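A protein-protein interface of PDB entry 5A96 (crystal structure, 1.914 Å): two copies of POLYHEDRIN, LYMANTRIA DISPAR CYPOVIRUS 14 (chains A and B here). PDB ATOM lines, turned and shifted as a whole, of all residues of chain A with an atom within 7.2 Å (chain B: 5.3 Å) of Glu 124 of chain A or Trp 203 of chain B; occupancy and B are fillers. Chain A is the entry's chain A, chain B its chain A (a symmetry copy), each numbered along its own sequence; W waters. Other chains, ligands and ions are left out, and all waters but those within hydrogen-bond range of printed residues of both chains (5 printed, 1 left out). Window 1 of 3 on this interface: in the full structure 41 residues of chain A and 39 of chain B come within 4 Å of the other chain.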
ATOM      1  N   GLU A  54     -20.055  26.194  16.419  1.00  0.00           N
ATOM      2  CA  GLU A  54     -21.123  26.135  17.411  1.00  0.00           C
ATOM      3  C   GLU A  54     -20.696  25.458  18.721  1.00  0.00           C
ATOM      4  O   GLU A  54     -19.944  24.486  18.722  1.00  0.00           O
ATOM      5  CB  GLU A  54     -22.324  25.370  16.849  1.00  0.00           C
ATOM      6  CG  GLU A  54     -22.921  25.958  15.597  1.00  0.00           C
ATOM      7  CD  GLU A  54     -23.827  27.147  15.877  1.00  0.00           C
ATOM      8  OE1 GLU A  54     -24.016  27.488  17.061  1.00  0.00           O
ATOM      9  OE2 GLU A  54     -24.351  27.740  14.906  1.00  0.00           O
ATOM     10  N   THR A  55     -21.204  25.977  19.833  1.00  0.00           N
ATOM     11  CA  THR A  55     -21.163  25.265  21.105  1.00  0.00           C
ATOM     12  C   THR A  55     -22.512  24.598  21.350  1.00  0.00           C
ATOM     13  O   THR A  55     -23.566  25.231  21.215  1.00  0.00           O
ATOM     14  CB  THR A  55     -20.871  26.225  22.260  1.00  0.00           C
ATOM     15  OG1 THR A  55     -19.519  26.695  22.150  1.00  0.00           O
ATOM     16  CG2 THR A  55     -21.078  25.535  23.622  1.00  0.00           C
ATOM     17  N   LEU A  56     -22.473  23.314  21.679  1.00  0.00           N
ATOM     18  CA  LEU A  56     -23.621  22.615  22.244  1.00  0.00           C
ATOM     19  C   LEU A  56     -23.410  22.487  23.757  1.00  0.00           C
ATOM     20  O   LEU A  56     -22.598  21.669  24.217  1.00  0.00           O
ATOM     21  CB  LEU A  56     -23.764  21.235  21.599  1.00  0.00           C
ATOM     22  CG  LEU A  56     -24.086  21.308  20.102  1.00  0.00           C
ATOM     23  CD1 LEU A  56     -24.193  19.919  19.470  1.00  0.00           C
ATOM     24  CD2 LEU A  56     -25.372  22.084  19.853  1.00  0.00           C
ATOM     25  N   ASP A  57     -24.116  23.321  24.523  1.00  0.00           N
ATOM     26  CA  ASP A  57     -23.988  23.329  25.975  1.00  0.00           C
ATOM     27  C   ASP A  57     -24.648  22.077  26.533  1.00  0.00           C
ATOM     28  O   ASP A  57     -25.313  21.340  25.816  1.00  0.00           O
ATOM     29  CB  ASP A  57     -24.638  24.593  26.582  1.00  0.00           C
ATOM     30  CG  ASP A  57     -23.893  25.111  27.841  1.00  0.00           C
ATOM     31  OD1 ASP A  57     -23.369  24.282  28.633  1.00  0.00           O
ATOM     32  OD2 ASP A  57     -23.832  26.357  28.039  1.00  0.00           O
ATOM     33  N   TYR A  58     -24.433  21.837  27.817  1.00  0.00           N
ATOM     34  CA  TYR A  58     -25.061  20.736  28.537  1.00  0.00           C
ATOM     35  C   TYR A  58     -26.573  20.672  28.306  1.00  0.00           C
ATOM     36  O   TYR A  58     -27.131  19.597  28.051  1.00  0.00           O
ATOM     37  CB  TYR A  58     -24.756  20.876  30.030  1.00  0.00           C
ATOM     38  CG  TYR A  58     -25.297  19.752  30.881  1.00  0.00           C
ATOM     39  CD1 TYR A  58     -24.655  18.514  30.931  1.00  0.00           C
ATOM     40  CD2 TYR A  58     -26.451  19.925  31.644  1.00  0.00           C
ATOM     41  CE1 TYR A  58     -25.153  17.473  31.714  1.00  0.00           C
ATOM     42  CE2 TYR A  58     -26.944  18.903  32.434  1.00  0.00           C
ATOM     43  CZ  TYR A  58     -26.289  17.677  32.461  1.00  0.00           C
ATOM     44  OH  TYR A  58     -26.781  16.658  33.248  1.00  0.00           O
ATOM     45  N   ASN A 118     -14.581  19.004  19.936  1.00  0.00           N
ATOM     46  CA  ASN A 118     -13.993  19.192  21.246  1.00  0.00           C
ATOM     47  C   ASN A 118     -15.083  18.978  22.293  1.00  0.00           C
ATOM     48  O   ASN A 118     -15.930  19.852  22.510  1.00  0.00           O
ATOM     49  CB  ASN A 118     -13.408  20.614  21.332  1.00  0.00           C
ATOM     50  CG  ASN A 118     -12.524  20.823  22.555  1.00  0.00           C
ATOM     51  OD1 ASN A 118     -12.597  20.080  23.535  1.00  0.00           O
ATOM     52  ND2 ASN A 118     -11.695  21.852  22.507  1.00  0.00           N
ATOM     53  N   ILE A 119     -15.069  17.800  22.915  1.00  0.00           N
ATOM     54  CA  ILE A 119     -16.040  17.443  23.941  1.00  0.00           C
ATOM     55  C   ILE A 119     -15.397  17.623  25.298  1.00  0.00           C
ATOM     56  O   ILE A 119     -14.311  17.101  25.544  1.00  0.00           O
ATOM     57  CB  ILE A 119     -16.483  15.968  23.822  1.00  0.00           C
ATOM     58  CG1 ILE A 119     -17.015  15.673  22.417  1.00  0.00           C
ATOM     59  CG2 ILE A 119     -17.554  15.637  24.893  1.00  0.00           C
ATOM     60  CD1 ILE A 119     -17.489  14.228  22.224  1.00  0.00           C
ATOM     61  N   GLN A 120     -16.095  18.308  26.186  1.00  0.00           N
ATOM     62  CA  GLN A 120     -15.598  18.596  27.520  1.00  0.00           C
ATOM     63  C   GLN A 120     -16.676  18.256  28.544  1.00  0.00           C
ATOM     64  O   GLN A 120     -17.792  17.908  28.182  1.00  0.00           O
ATOM     65  CB  GLN A 120     -15.183  20.063  27.642  1.00  0.00           C
ATOM     66  CG  GLN A 120     -14.036  20.461  26.726  1.00  0.00           C
ATOM     67  CD  GLN A 120     -12.729  19.800  27.106  1.00  0.00           C
ATOM     68  OE1 GLN A 120     -12.502  19.469  28.267  1.00  0.00           O
ATOM     69  NE2 GLN A 120     -11.863  19.606  26.128  1.00  0.00           N
ATOM     70  N   GLY A 121     -16.319  18.298  29.819  1.00  0.00           N
ATOM     71  CA  GLY A 121     -17.307  18.172  30.867  1.00  0.00           C
ATOM     72  C   GLY A 121     -18.141  19.438  30.966  1.00  0.00           C
ATOM     73  O   GLY A 121     -18.139  20.295  30.065  1.00  0.00           O
ATOM     74  N   TYR A 122     -18.840  19.571  32.084  1.00  0.00           N
ATOM     75  CA  TYR A 122     -19.844  20.600  32.249  1.00  0.00           C
ATOM     76  C   TYR A 122     -19.252  21.999  32.145  1.00  0.00           C
ATOM     77  O   TYR A 122     -19.887  22.911  31.624  1.00  0.00           O
ATOM     78  CB  TYR A 122     -20.507  20.429  33.618  1.00  0.00           C
ATOM     79  CG  TYR A 122     -21.713  21.309  33.846  1.00  0.00           C
ATOM     80  CD1 TYR A 122     -22.926  21.051  33.208  1.00  0.00           C
ATOM     81  CD2 TYR A 122     -21.649  22.391  34.714  1.00  0.00           C
ATOM     82  CE1 TYR A 122     -24.045  21.860  33.430  1.00  0.00           C
ATOM     83  CE2 TYR A 122     -22.756  23.198  34.944  1.00  0.00           C
ATOM     84  CZ  TYR A 122     -23.948  22.929  34.300  1.00  0.00           C
ATOM     85  OH  TYR A 122     -25.033  23.739  34.535  1.00  0.00           O
ATOM     86  N   ASP A 123     -18.035  22.173  32.646  1.00  0.00           N
ATOM     87  CA  ASP A 123     -17.456  23.513  32.761  1.00  0.00           C
ATOM     88  C   ASP A 123     -16.803  24.021  31.467  1.00  0.00           C
ATOM     89  O   ASP A 123     -16.426  25.182  31.386  1.00  0.00           O
ATOM     90  CB  ASP A 123     -16.451  23.545  33.910  1.00  0.00           C
ATOM     91  CG  ASP A 123     -17.092  23.245  35.262  1.00  0.00           C
ATOM     92  OD1 ASP A 123     -18.323  23.414  35.408  1.00  0.00           O
ATOM     93  OD2 ASP A 123     -16.361  22.836  36.188  1.00  0.00           O
ATOM     94  N   GLU A 124     -16.667  23.144  30.475  1.00  0.00           N
ATOM     95  CA  GLU A 124     -16.105  23.488  29.164  1.00  0.00           C
ATOM     96  C   GLU A 124     -14.617  23.794  29.220  1.00  0.00           C
ATOM     97  O   GLU A 124     -14.062  24.336  28.264  1.00  0.00           O
ATOM     98  CB  GLU A 124     -16.838  24.676  28.542  1.00  0.00           C
ATOM     99  CG  GLU A 124     -18.328  24.451  28.407  1.00  0.00           C
ATOM    100  CD  GLU A 124     -19.031  25.568  27.696  1.00  0.00           C
ATOM    101  OE1 GLU A 124     -18.431  26.663  27.540  1.00  0.00           O
ATOM    102  OE2 GLU A 124     -20.194  25.342  27.302  1.00  0.00           O
ATOM    103  N   ILE A 125     -13.974  23.445  30.329  1.00  0.00           N
ATOM    104  CA  ILE A 125     -12.580  23.830  30.539  1.00  0.00           C
ATOM    105  C   ILE A 125     -11.613  22.655  30.396  1.00  0.00           C
ATOM    106  O   ILE A 125     -11.535  21.779  31.260  1.00  0.00           O
ATOM    107  CB  ILE A 125     -12.391  24.522  31.923  1.00  0.00           C
ATOM    108  CG1 ILE A 125     -13.077  25.893  31.906  1.00  0.00           C
ATOM    109  CG2 ILE A 125     -10.895  24.672  32.260  1.00  0.00           C
ATOM    110  CD1 ILE A 125     -13.361  26.506  33.282  1.00  0.00           C
ATOM    111  N   GLU A 126     -10.865  22.668  29.294  1.00  0.00           N
ATOM    112  CA  GLU A 126      -9.841  21.663  29.021  1.00  0.00           C
ATOM    113  C   GLU A 126      -8.696  21.736  30.036  1.00  0.00           C
ATOM    114  O   GLU A 126      -8.263  22.825  30.427  1.00  0.00           O
ATOM    115  CB  GLU A 126      -9.286  21.896  27.613  1.00  0.00           C
ATOM    116  CG  GLU A 126      -8.432  20.763  27.080  1.00  0.00           C
ATOM    117  CD  GLU A 126      -7.012  20.735  27.642  1.00  0.00           C
ATOM    118  OE1 GLU A 126      -6.470  21.800  28.004  1.00  0.00           O
ATOM    119  OE2 GLU A 126      -6.429  19.632  27.702  1.00  0.00           O
ATOM    120  N   SER A 133      -5.484  25.640  29.708  1.00  0.00           N
ATOM    121  CA  SER A 133      -6.322  25.035  28.679  1.00  0.00           C
ATOM    122  C   SER A 133      -5.707  25.236  27.291  1.00  0.00           C
ATOM    123  O   SER A 133      -5.257  26.328  26.958  1.00  0.00           O
ATOM    124  CB  SER A 133      -7.725  25.650  28.679  1.00  0.00           C
ATOM    125  OG  SER A 133      -8.407  25.408  29.899  1.00  0.00           O
ATOM    126  N   ASN A 134      -5.715  24.186  26.477  1.00  0.00           N
ATOM    127  CA  ASN A 134      -5.262  24.286  25.095  1.00  0.00           C
ATOM    128  C   ASN A 134      -6.465  24.493  24.192  1.00  0.00           C
ATOM    129  O   ASN A 134      -7.508  23.877  24.417  1.00  0.00           O
ATOM    130  CB  ASN A 134      -4.533  23.008  24.693  1.00  0.00           C
ATOM    131  CG  ASN A 134      -3.215  22.844  25.415  1.00  0.00           C
ATOM    132  OD1 ASN A 134      -2.539  23.820  25.707  1.00  0.00           O
ATOM    133  ND2 ASN A 134      -2.846  21.610  25.709  1.00  0.00           N
ATOM    134  N   VAL A 135      -6.343  25.346  23.175  1.00  0.00           N
ATOM    135  CA  VAL A 135      -7.492  25.600  22.309  1.00  0.00           C
ATOM    136  C   VAL A 135      -7.789  24.365  21.459  1.00  0.00           C
ATOM    137  O   VAL A 135      -8.911  24.174  21.011  1.00  0.00           O
ATOM    138  CB  VAL A 135      -7.313  26.856  21.423  1.00  0.00           C
ATOM    139  CG1 VAL A 135      -7.228  28.110  22.289  1.00  0.00           C
ATOM    140  CG2 VAL A 135      -6.091  26.729  20.532  1.00  0.00           C
ATOM    141  N   PRO A 137      -7.016  20.474  22.166  1.00  0.00           N
ATOM    142  CA  PRO A 137      -6.458  19.259  22.777  1.00  0.00           C
ATOM    143  C   PRO A 137      -6.342  18.157  21.717  1.00  0.00           C
ATOM    144  O   PRO A 137      -7.038  18.227  20.712  1.00  0.00           O
ATOM    145  CB  PRO A 137      -7.480  18.898  23.865  1.00  0.00           C
ATOM    146  CG  PRO A 137      -8.762  19.552  23.430  1.00  0.00           C
ATOM    147  CD  PRO A 137      -8.370  20.791  22.650  1.00  0.00           C
ATOM    148  N   HIS A 170     -21.163  14.325  31.249  1.00  0.00           N
ATOM    149  CA  HIS A 170     -21.908  15.561  31.461  1.00  0.00           C
ATOM    150  C   HIS A 170     -21.388  16.506  30.404  1.00  0.00           C
ATOM    151  O   HIS A 170     -20.702  17.485  30.726  1.00  0.00           O
ATOM    152  CB  HIS A 170     -21.645  16.126  32.860  1.00  0.00           C
ATOM    153  CG  HIS A 170     -21.532  15.076  33.921  1.00  0.00           C
ATOM    154  ND1 HIS A 170     -22.614  14.344  34.354  1.00  0.00           N
ATOM    155  CD2 HIS A 170     -20.467  14.618  34.620  1.00  0.00           C
ATOM    156  CE1 HIS A 170     -22.228  13.486  35.282  1.00  0.00           C
ATOM    157  NE2 HIS A 170     -20.925  13.623  35.452  1.00  0.00           N
ATOM    158  N   PRO A 171     -21.687  16.198  29.127  1.00  0.00           N
ATOM    159  CA  PRO A 171     -20.947  16.814  28.024  1.00  0.00           C
ATOM    160  C   PRO A 171     -21.322  18.246  27.714  1.00  0.00           C
ATOM    161  O   PRO A 171     -22.441  18.693  27.956  1.00  0.00           O
ATOM    162  CB  PRO A 171     -21.290  15.924  26.823  1.00  0.00           C
ATOM    163  CG  PRO A 171     -22.675  15.415  27.123  1.00  0.00           C
ATOM    164  CD  PRO A 171     -22.670  15.209  28.641  1.00  0.00           C
ATOM    165  N   THR A 172     -20.323  18.955  27.212  1.00  0.00           N
ATOM    166  CA  THR A 172     -20.495  20.138  26.392  1.00  0.00           C
ATOM    167  C   THR A 172     -19.606  19.863  25.177  1.00  0.00           C
ATOM    168  O   THR A 172     -18.666  19.061  25.268  1.00  0.00           O
ATOM    169  CB  THR A 172     -20.001  21.400  27.111  1.00  0.00           C
ATOM    170  OG1 THR A 172     -18.607  21.262  27.394  1.00  0.00           O
ATOM    171  CG2 THR A 172     -20.768  21.608  28.426  1.00  0.00           C
ATOM    172  N   MET A 173     -19.876  20.484  24.035  1.00  0.00           N
ATOM    173  CA  MET A 173     -18.949  20.316  22.918  1.00  0.00           C
ATOM    174  C   MET A 173     -18.948  21.518  22.003  1.00  0.00           C
ATOM    175  O   MET A 173     -19.973  22.170  21.812  1.00  0.00           O
ATOM    176  CB  MET A 173     -19.235  19.025  22.112  1.00  0.00           C
ATOM    177  CG  MET A 173     -20.358  19.122  21.090  1.00  0.00           C
ATOM    178  SD  MET A 173     -20.537  17.641  20.029  1.00  0.00           S
ATOM    179  CE  MET A 173     -20.850  16.400  21.294  1.00  0.00           C
ATOM    180  N   ALA A 174     -17.770  21.800  21.459  1.00  0.00           N
ATOM    181  CA  ALA A 174     -17.593  22.804  20.433  1.00  0.00           C
ATOM    182  C   ALA A 174     -17.295  22.066  19.136  1.00  0.00           C
ATOM    183  O   ALA A 174     -16.419  21.191  19.080  1.00  0.00           O
ATOM    184  CB  ALA A 174     -16.441  23.743  20.792  1.00  0.00           C
ATOM    185  N   VAL A 175     -18.058  22.389  18.106  1.00  0.00           N
ATOM    186  CA  VAL A 175     -17.846  21.803  16.791  1.00  0.00           C
ATOM    187  C   VAL A 175     -17.597  22.912  15.772  1.00  0.00           C
ATOM    188  O   VAL A 175     -18.367  23.872  15.704  1.00  0.00           O
ATOM    189  CB  VAL A 175     -19.094  21.012  16.352  1.00  0.00           C
ATOM    190  CG1 VAL A 175     -18.854  20.341  15.015  1.00  0.00           C
ATOM    191  CG2 VAL A 175     -19.486  19.987  17.433  1.00  0.00           C
ATOM    192  N   TYR B  27      -6.548  30.301  25.362  1.00  0.00           N
ATOM    193  CA  TYR B  27      -7.753  31.109  25.221  1.00  0.00           C
ATOM    194  C   TYR B  27      -7.586  32.472  25.900  1.00  0.00           C
ATOM    195  O   TYR B  27      -6.768  32.632  26.785  1.00  0.00           O
ATOM    196  CB  TYR B  27      -8.945  30.409  25.882  1.00  0.00           C
ATOM    197  CG  TYR B  27      -9.485  29.175  25.187  1.00  0.00           C
ATOM    198  CD1 TYR B  27     -10.490  29.283  24.238  1.00  0.00           C
ATOM    199  CD2 TYR B  27      -9.040  27.897  25.532  1.00  0.00           C
ATOM    200  CE1 TYR B  27     -11.015  28.170  23.614  1.00  0.00           C
ATOM    201  CE2 TYR B  27      -9.568  26.763  24.908  1.00  0.00           C
ATOM    202  CZ  TYR B  27     -10.552  26.911  23.954  1.00  0.00           C
ATOM    203  OH  TYR B  27     -11.093  25.805  23.330  1.00  0.00           O
ATOM    204  N   LYS B  45     -18.597  32.631  32.011  1.00  0.00           N
ATOM    205  CA  LYS B  45     -17.342  32.603  31.270  1.00  0.00           C
ATOM    206  C   LYS B  45     -17.612  32.978  29.815  1.00  0.00           C
ATOM    207  O   LYS B  45     -18.432  32.327  29.147  1.00  0.00           O
ATOM    208  CB  LYS B  45     -16.723  31.210  31.338  1.00  0.00           C
ATOM    209  CG  LYS B  45     -15.757  30.909  30.196  1.00  0.00           C
ATOM    210  CD  LYS B  45     -15.140  29.535  30.369  1.00  0.00           C
ATOM    211  CE  LYS B  45     -16.174  28.429  30.139  1.00  0.00           C
ATOM    212  NZ  LYS B  45     -16.474  28.209  28.692  1.00  0.00           N
ATOM    213  N   THR B  47     -15.240  33.379  26.330  1.00  0.00           N
ATOM    214  CA  THR B  47     -13.932  32.839  25.966  1.00  0.00           C
ATOM    215  C   THR B  47     -13.811  32.580  24.471  1.00  0.00           C
ATOM    216  O   THR B  47     -14.784  32.277  23.777  1.00  0.00           O
ATOM    217  CB  THR B  47     -13.603  31.528  26.745  1.00  0.00           C
ATOM    218  OG1 THR B  47     -12.204  31.233  26.637  1.00  0.00           O
ATOM    219  CG2 THR B  47     -14.411  30.340  26.218  1.00  0.00           C
ATOM    220  N   ASN B  48     -12.590  32.698  23.984  1.00  0.00           N
ATOM    221  CA  ASN B  48     -12.321  32.511  22.578  1.00  0.00           C
ATOM    222  C   ASN B  48     -10.816  32.404  22.374  1.00  0.00           C
ATOM    223  O   ASN B  48     -10.041  32.874  23.207  1.00  0.00           O
ATOM    224  CB  ASN B  48     -12.890  33.688  21.771  1.00  0.00           C
ATOM    225  CG  ASN B  48     -12.966  33.393  20.290  1.00  0.00           C
ATOM    226  OD1 ASN B  48     -12.052  33.714  19.522  1.00  0.00           O
ATOM    227  ND2 ASN B  48     -14.052  32.756  19.879  1.00  0.00           N
ATOM    228  N   GLU B  54     -19.810  39.003  23.200  1.00  0.00           N
ATOM    229  CA  GLU B  54     -21.018  38.404  23.759  1.00  0.00           C
ATOM    230  C   GLU B  54     -22.003  39.438  24.320  1.00  0.00           C
ATOM    231  O   GLU B  54     -21.609  40.440  24.912  1.00  0.00           O
ATOM    232  CB  GLU B  54     -20.653  37.434  24.884  1.00  0.00           C
ATOM    233  CG  GLU B  54     -19.749  36.299  24.477  1.00  0.00           C
ATOM    234  CD  GLU B  54     -20.493  35.177  23.770  1.00  0.00           C
ATOM    235  OE1 GLU B  54     -21.729  35.273  23.632  1.00  0.00           O
ATOM    236  OE2 GLU B  54     -19.837  34.195  23.352  1.00  0.00           O
ATOM    237  N   ASN B 201     -17.407  30.646  17.742  1.00  0.00           N
ATOM    238  CA  ASN B 201     -18.234  30.191  18.861  1.00  0.00           C
ATOM    239  C   ASN B 201     -17.553  29.090  19.684  1.00  0.00           C
ATOM    240  O   ASN B 201     -18.209  28.186  20.188  1.00  0.00           O
ATOM    241  CB  ASN B 201     -19.619  29.730  18.375  1.00  0.00           C
ATOM    242  CG  ASN B 201     -20.503  30.892  17.936  1.00  0.00           C
ATOM    243  OD1 ASN B 201     -20.534  31.936  18.587  1.00  0.00           O
ATOM    244  ND2 ASN B 201     -21.206  30.720  16.826  1.00  0.00           N
ATOM    245  N   PHE B 202     -16.237  29.183  19.815  1.00  0.00           N
ATOM    246  CA  PHE B 202     -15.485  28.330  20.722  1.00  0.00           C
ATOM    247  C   PHE B 202     -15.010  29.210  21.868  1.00  0.00           C
ATOM    248  O   PHE B 202     -13.912  29.760  21.764  1.00  0.00           O
ATOM    249  CB  PHE B 202     -14.204  27.817  20.060  1.00  0.00           C
ATOM    250  CG  PHE B 202     -14.395  26.717  19.053  1.00  0.00           C
ATOM    251  CD1 PHE B 202     -15.541  26.620  18.289  1.00  0.00           C
ATOM    252  CD2 PHE B 202     -13.380  25.788  18.855  1.00  0.00           C
ATOM    253  CE1 PHE B 202     -15.678  25.600  17.349  1.00  0.00           C
ATOM    254  CE2 PHE B 202     -13.510  24.768  17.924  1.00  0.00           C
ATOM    255  CZ  PHE B 202     -14.664  24.677  17.168  1.00  0.00           C
ATOM    256  N   TRP B 203     -15.768  29.370  22.951  1.00  0.00           N
ATOM    257  CA  TRP B 203     -17.035  28.695  23.229  1.00  0.00           C
ATOM    258  C   TRP B 203     -18.153  29.721  23.412  1.00  0.00           C
ATOM    259  O   TRP B 203     -17.895  30.873  23.715  1.00  0.00           O
ATOM    260  CB  TRP B 203     -16.889  27.905  24.536  1.00  0.00           C
ATOM    261  CG  TRP B 203     -15.881  26.792  24.445  1.00  0.00           C
ATOM    262  CD1 TRP B 203     -14.532  26.922  24.286  1.00  0.00           C
ATOM    263  CD2 TRP B 203     -16.142  25.381  24.501  1.00  0.00           C
ATOM    264  NE1 TRP B 203     -13.937  25.685  24.241  1.00  0.00           N
ATOM    265  CE2 TRP B 203     -14.902  24.721  24.370  1.00  0.00           C
ATOM    266  CE3 TRP B 203     -17.302  24.611  24.650  1.00  0.00           C
ATOM    267  CZ2 TRP B 203     -14.788  23.331  24.374  1.00  0.00           C
ATOM    268  CZ3 TRP B 203     -17.186  23.231  24.661  1.00  0.00           C
ATOM    269  CH2 TRP B 203     -15.937  22.605  24.529  1.00  0.00           C
ATOM    270  N   ALA B 204     -19.406  29.306  23.262  1.00  0.00           N
ATOM    271  CA  ALA B 204     -20.503  30.218  23.510  1.00  0.00           C
ATOM    272  C   ALA B 204     -20.498  30.537  24.998  1.00  0.00           C
ATOM    273  O   ALA B 204     -19.967  29.762  25.798  1.00  0.00           O
ATOM    274  CB  ALA B 204     -21.826  29.600  23.088  1.00  0.00           C
ATOM    275  N   LYS B 205     -21.075  31.677  25.373  1.00  0.00           N
ATOM    276  CA  LYS B 205     -21.188  32.049  26.782  1.00  0.00           C
ATOM    277  C   LYS B 205     -21.743  30.903  27.646  1.00  0.00           C
ATOM    278  O   LYS B 205     -22.696  30.203  27.266  1.00  0.00           O
ATOM    279  CB  LYS B 205     -22.065  33.288  26.943  1.00  0.00           C
ATOM    280  CG  LYS B 205     -23.508  33.056  26.518  1.00  0.00           C
ATOM    281  CD  LYS B 205     -24.283  34.349  26.431  1.00  0.00           C
ATOM    282  CE  LYS B 205     -25.714  34.070  26.020  1.00  0.00           C
ATOM    283  NZ  LYS B 205     -26.434  35.293  25.603  1.00  0.00           N
ATOM    284  N   LYS B 206     -21.152  30.744  28.823  1.00  0.00           N
ATOM    285  CA  LYS B 206     -21.433  29.609  29.704  1.00  0.00           C
ATOM    286  C   LYS B 206     -21.568  30.107  31.136  1.00  0.00           C
ATOM    287  O   LYS B 206     -20.732  30.904  31.581  1.00  0.00           O
ATOM    288  CB  LYS B 206     -20.251  28.634  29.649  1.00  0.00           C
ATOM    289  CG  LYS B 206     -20.226  27.634  30.784  1.00  0.00           C
ATOM    290  CD  LYS B 206     -21.314  26.588  30.626  1.00  0.00           C
ATOM    291  CE  LYS B 206     -21.233  25.576  31.753  1.00  0.00           C
ATOM    292  NZ  LYS B 206     -22.171  24.438  31.551  1.00  0.00           N
HETATM  293  O   HOH W   1     -24.653  25.887  32.261  1.00  0.00           O
HETATM  294  O   HOH W   2     -10.295  23.337  24.507  1.00  0.00           O
HETATM  295  O   HOH W   3     -13.952  26.931  27.810  1.00  0.00           O
HETATM  296  O   HOH W   4      -5.923  28.818  27.841  1.00  0.00           O
HETATM  297  O   HOH W   5     -10.600  26.436  20.538  1.00  0.00           O
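O of Asn 201 of chain B lies within hydrogen-bond range of OG1 of Thr 55 of chain A.
The backbone carbonyl oxygen of Tyr 122 of chain A lies within hydrogen-bond range of the side-chain amino group of Lys 206 of chain B (2.7 Å).
OD1 of Asp 57 of chain A lies within salt-bridge range of NZ of Lys 206 of chain B (3.2 Å).
The backbone NH (N) of Ala 204 of chain B lies within hydrogen-bond range of the side-chain hydroxyl (OG1) of Thr 55 of chain A (2.8 Å).
OE1 of Glu 124 of chain A lies within salt-bridge range of NZ of Lys 45 of chain B (2.7 Å).
The side-chain hydroxyl (OH) of Tyr 27 of chain B sits at hydrogen-bond distance from the indole nitrogen (NE1) of Trp 203 of chain B, at 3.0 Å.
O of Thr 47 of chain B sits at hydrogen-bond distance from N of Trp 203 of chain B, 3.2 Å away.
N of Val 175 of chain A sits at hydrogen-bond distance from O of Glu 54 of chain A (2.9 Å).
Among the printed residues, pairs that only touch across the chains: Thr 55 of chain A with Trp 203 of chain B (3.4 Å), Glu 124 of chain A with Lys 206 of chain B (3.4 Å), Asn 118 of chain A with Trp 203 of chain B (3.4 Å), Asp 123 of chain A with Lys 45 of chain B (3.5 Å), Val 135 of chain A with Tyr 27 of chain B (3.5 Å), Ala 174 of chain A with Trp 203 of chain B (3.6 Å), Asn 134 of chain A with Tyr 27 of chain B (3.6 Å), Val 175 of chain A with Phe 202 of chain B (3.6 Å), Glu 124 of chain A with Trp 203 of chain B (3.6 Å), Gln 120 of chain A with Trp 203 of chain B (3.6 Å), Met 173 of chain A with Trp 203 of chain B (3.6 Å), Thr 172 of chain A with Trp 203 of chain B (3.7 Å), Glu 124 of chain A with Ala 204 of chain B (3.9 Å), Ala 174 of chain A with Phe 202 of chain B (3.9 Å) and Glu 54 of chain A with Asn 201 of chain B (3.97 Å).
Glu 124 of chain A touches just these residues of chain B: Lys 45 (2.7 Å), Trp 203 (3.6 Å), Ala 204 (3.9 Å) and Lys 206 (3.4 Å).
Of chain A, only Thr 55, Asn 118, Gln 120, Glu 124, Thr 172, Met 173 and Ala 174 come within 4 Å of Trp 203 of chain B.
Printed residues of chain B within 4 Å of Met 173 of chain A: Trp 203 (3.6 Å).
Of the printed residues of chain B, Asn 118 of chain A touches Trp 203.
Of the printed residues of chain B, Val 135 of chain A touches Tyr 27 (3.5 Å).
Of the printed residues of chain A, Lys 45 of chain B touches Asp 123 (3.5 Å) and Glu 124 (2.7 Å).
Glu 126 of chain A touches none of the printed residues of chain B.
The nearest printed residue of chain B that does not touch Glu 124 of chain A is Lys 205 of chain B (5.4 Å).
The nearest printed residue of chain B that does not touch Asp 123 of chain A is Lys 206 of chain B (4.4 Å).
Of the 11 printed residues of chain B, 7 touch a printed residue of chain A.
Printed residues of chain B that touch a printed residue of chain A: Tyr 27, Lys 45, Asn 201, Phe 202, Trp 203, Ala 204 and Lys 206.
Hydrophobic or aromatic side chains of chain B within 4 Å of the printed part of chain A: Tyr 27, Phe 202, Trp 203 and Ala 204.
Of the 24 printed residues of chain A, 14 touch a printed residue of chain B.
Hydrophobic or aromatic side chains of chain A within 4 Å of the printed part of chain B: Tyr 122, Val 135 and Ala 174.
Among the printed residues, 20 pairs touch across the chains.
Among the printed residues, Asp or Glu carboxylates within 4 Å of a Lys or Arg side-chain nitrogen of the other chain: Asp 57 of chain A with Lys 206 of chain B and Glu 124 of chain A with Lys 45 of chain B.
Position printed for both chains: 54.
Water W4 bridges O of Ser 133 of chain A (2.7 Å) and N of Tyr 27 of chain B (3.0 Å).
Water W2 lies within hydrogen-bond range of the backbone carbonyl oxygen of Asn 134 of chain A (2.8 Å), the side-chain hydroxyl of Tyr 27 of chain B (2.8 Å) and the side-chain amide nitrogen of Asn 118 of chain A (2.9 Å).
Water W1 lies within hydrogen-bond range of NZ of Lys 206 of chain B and OH of Tyr 122 of chain A.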
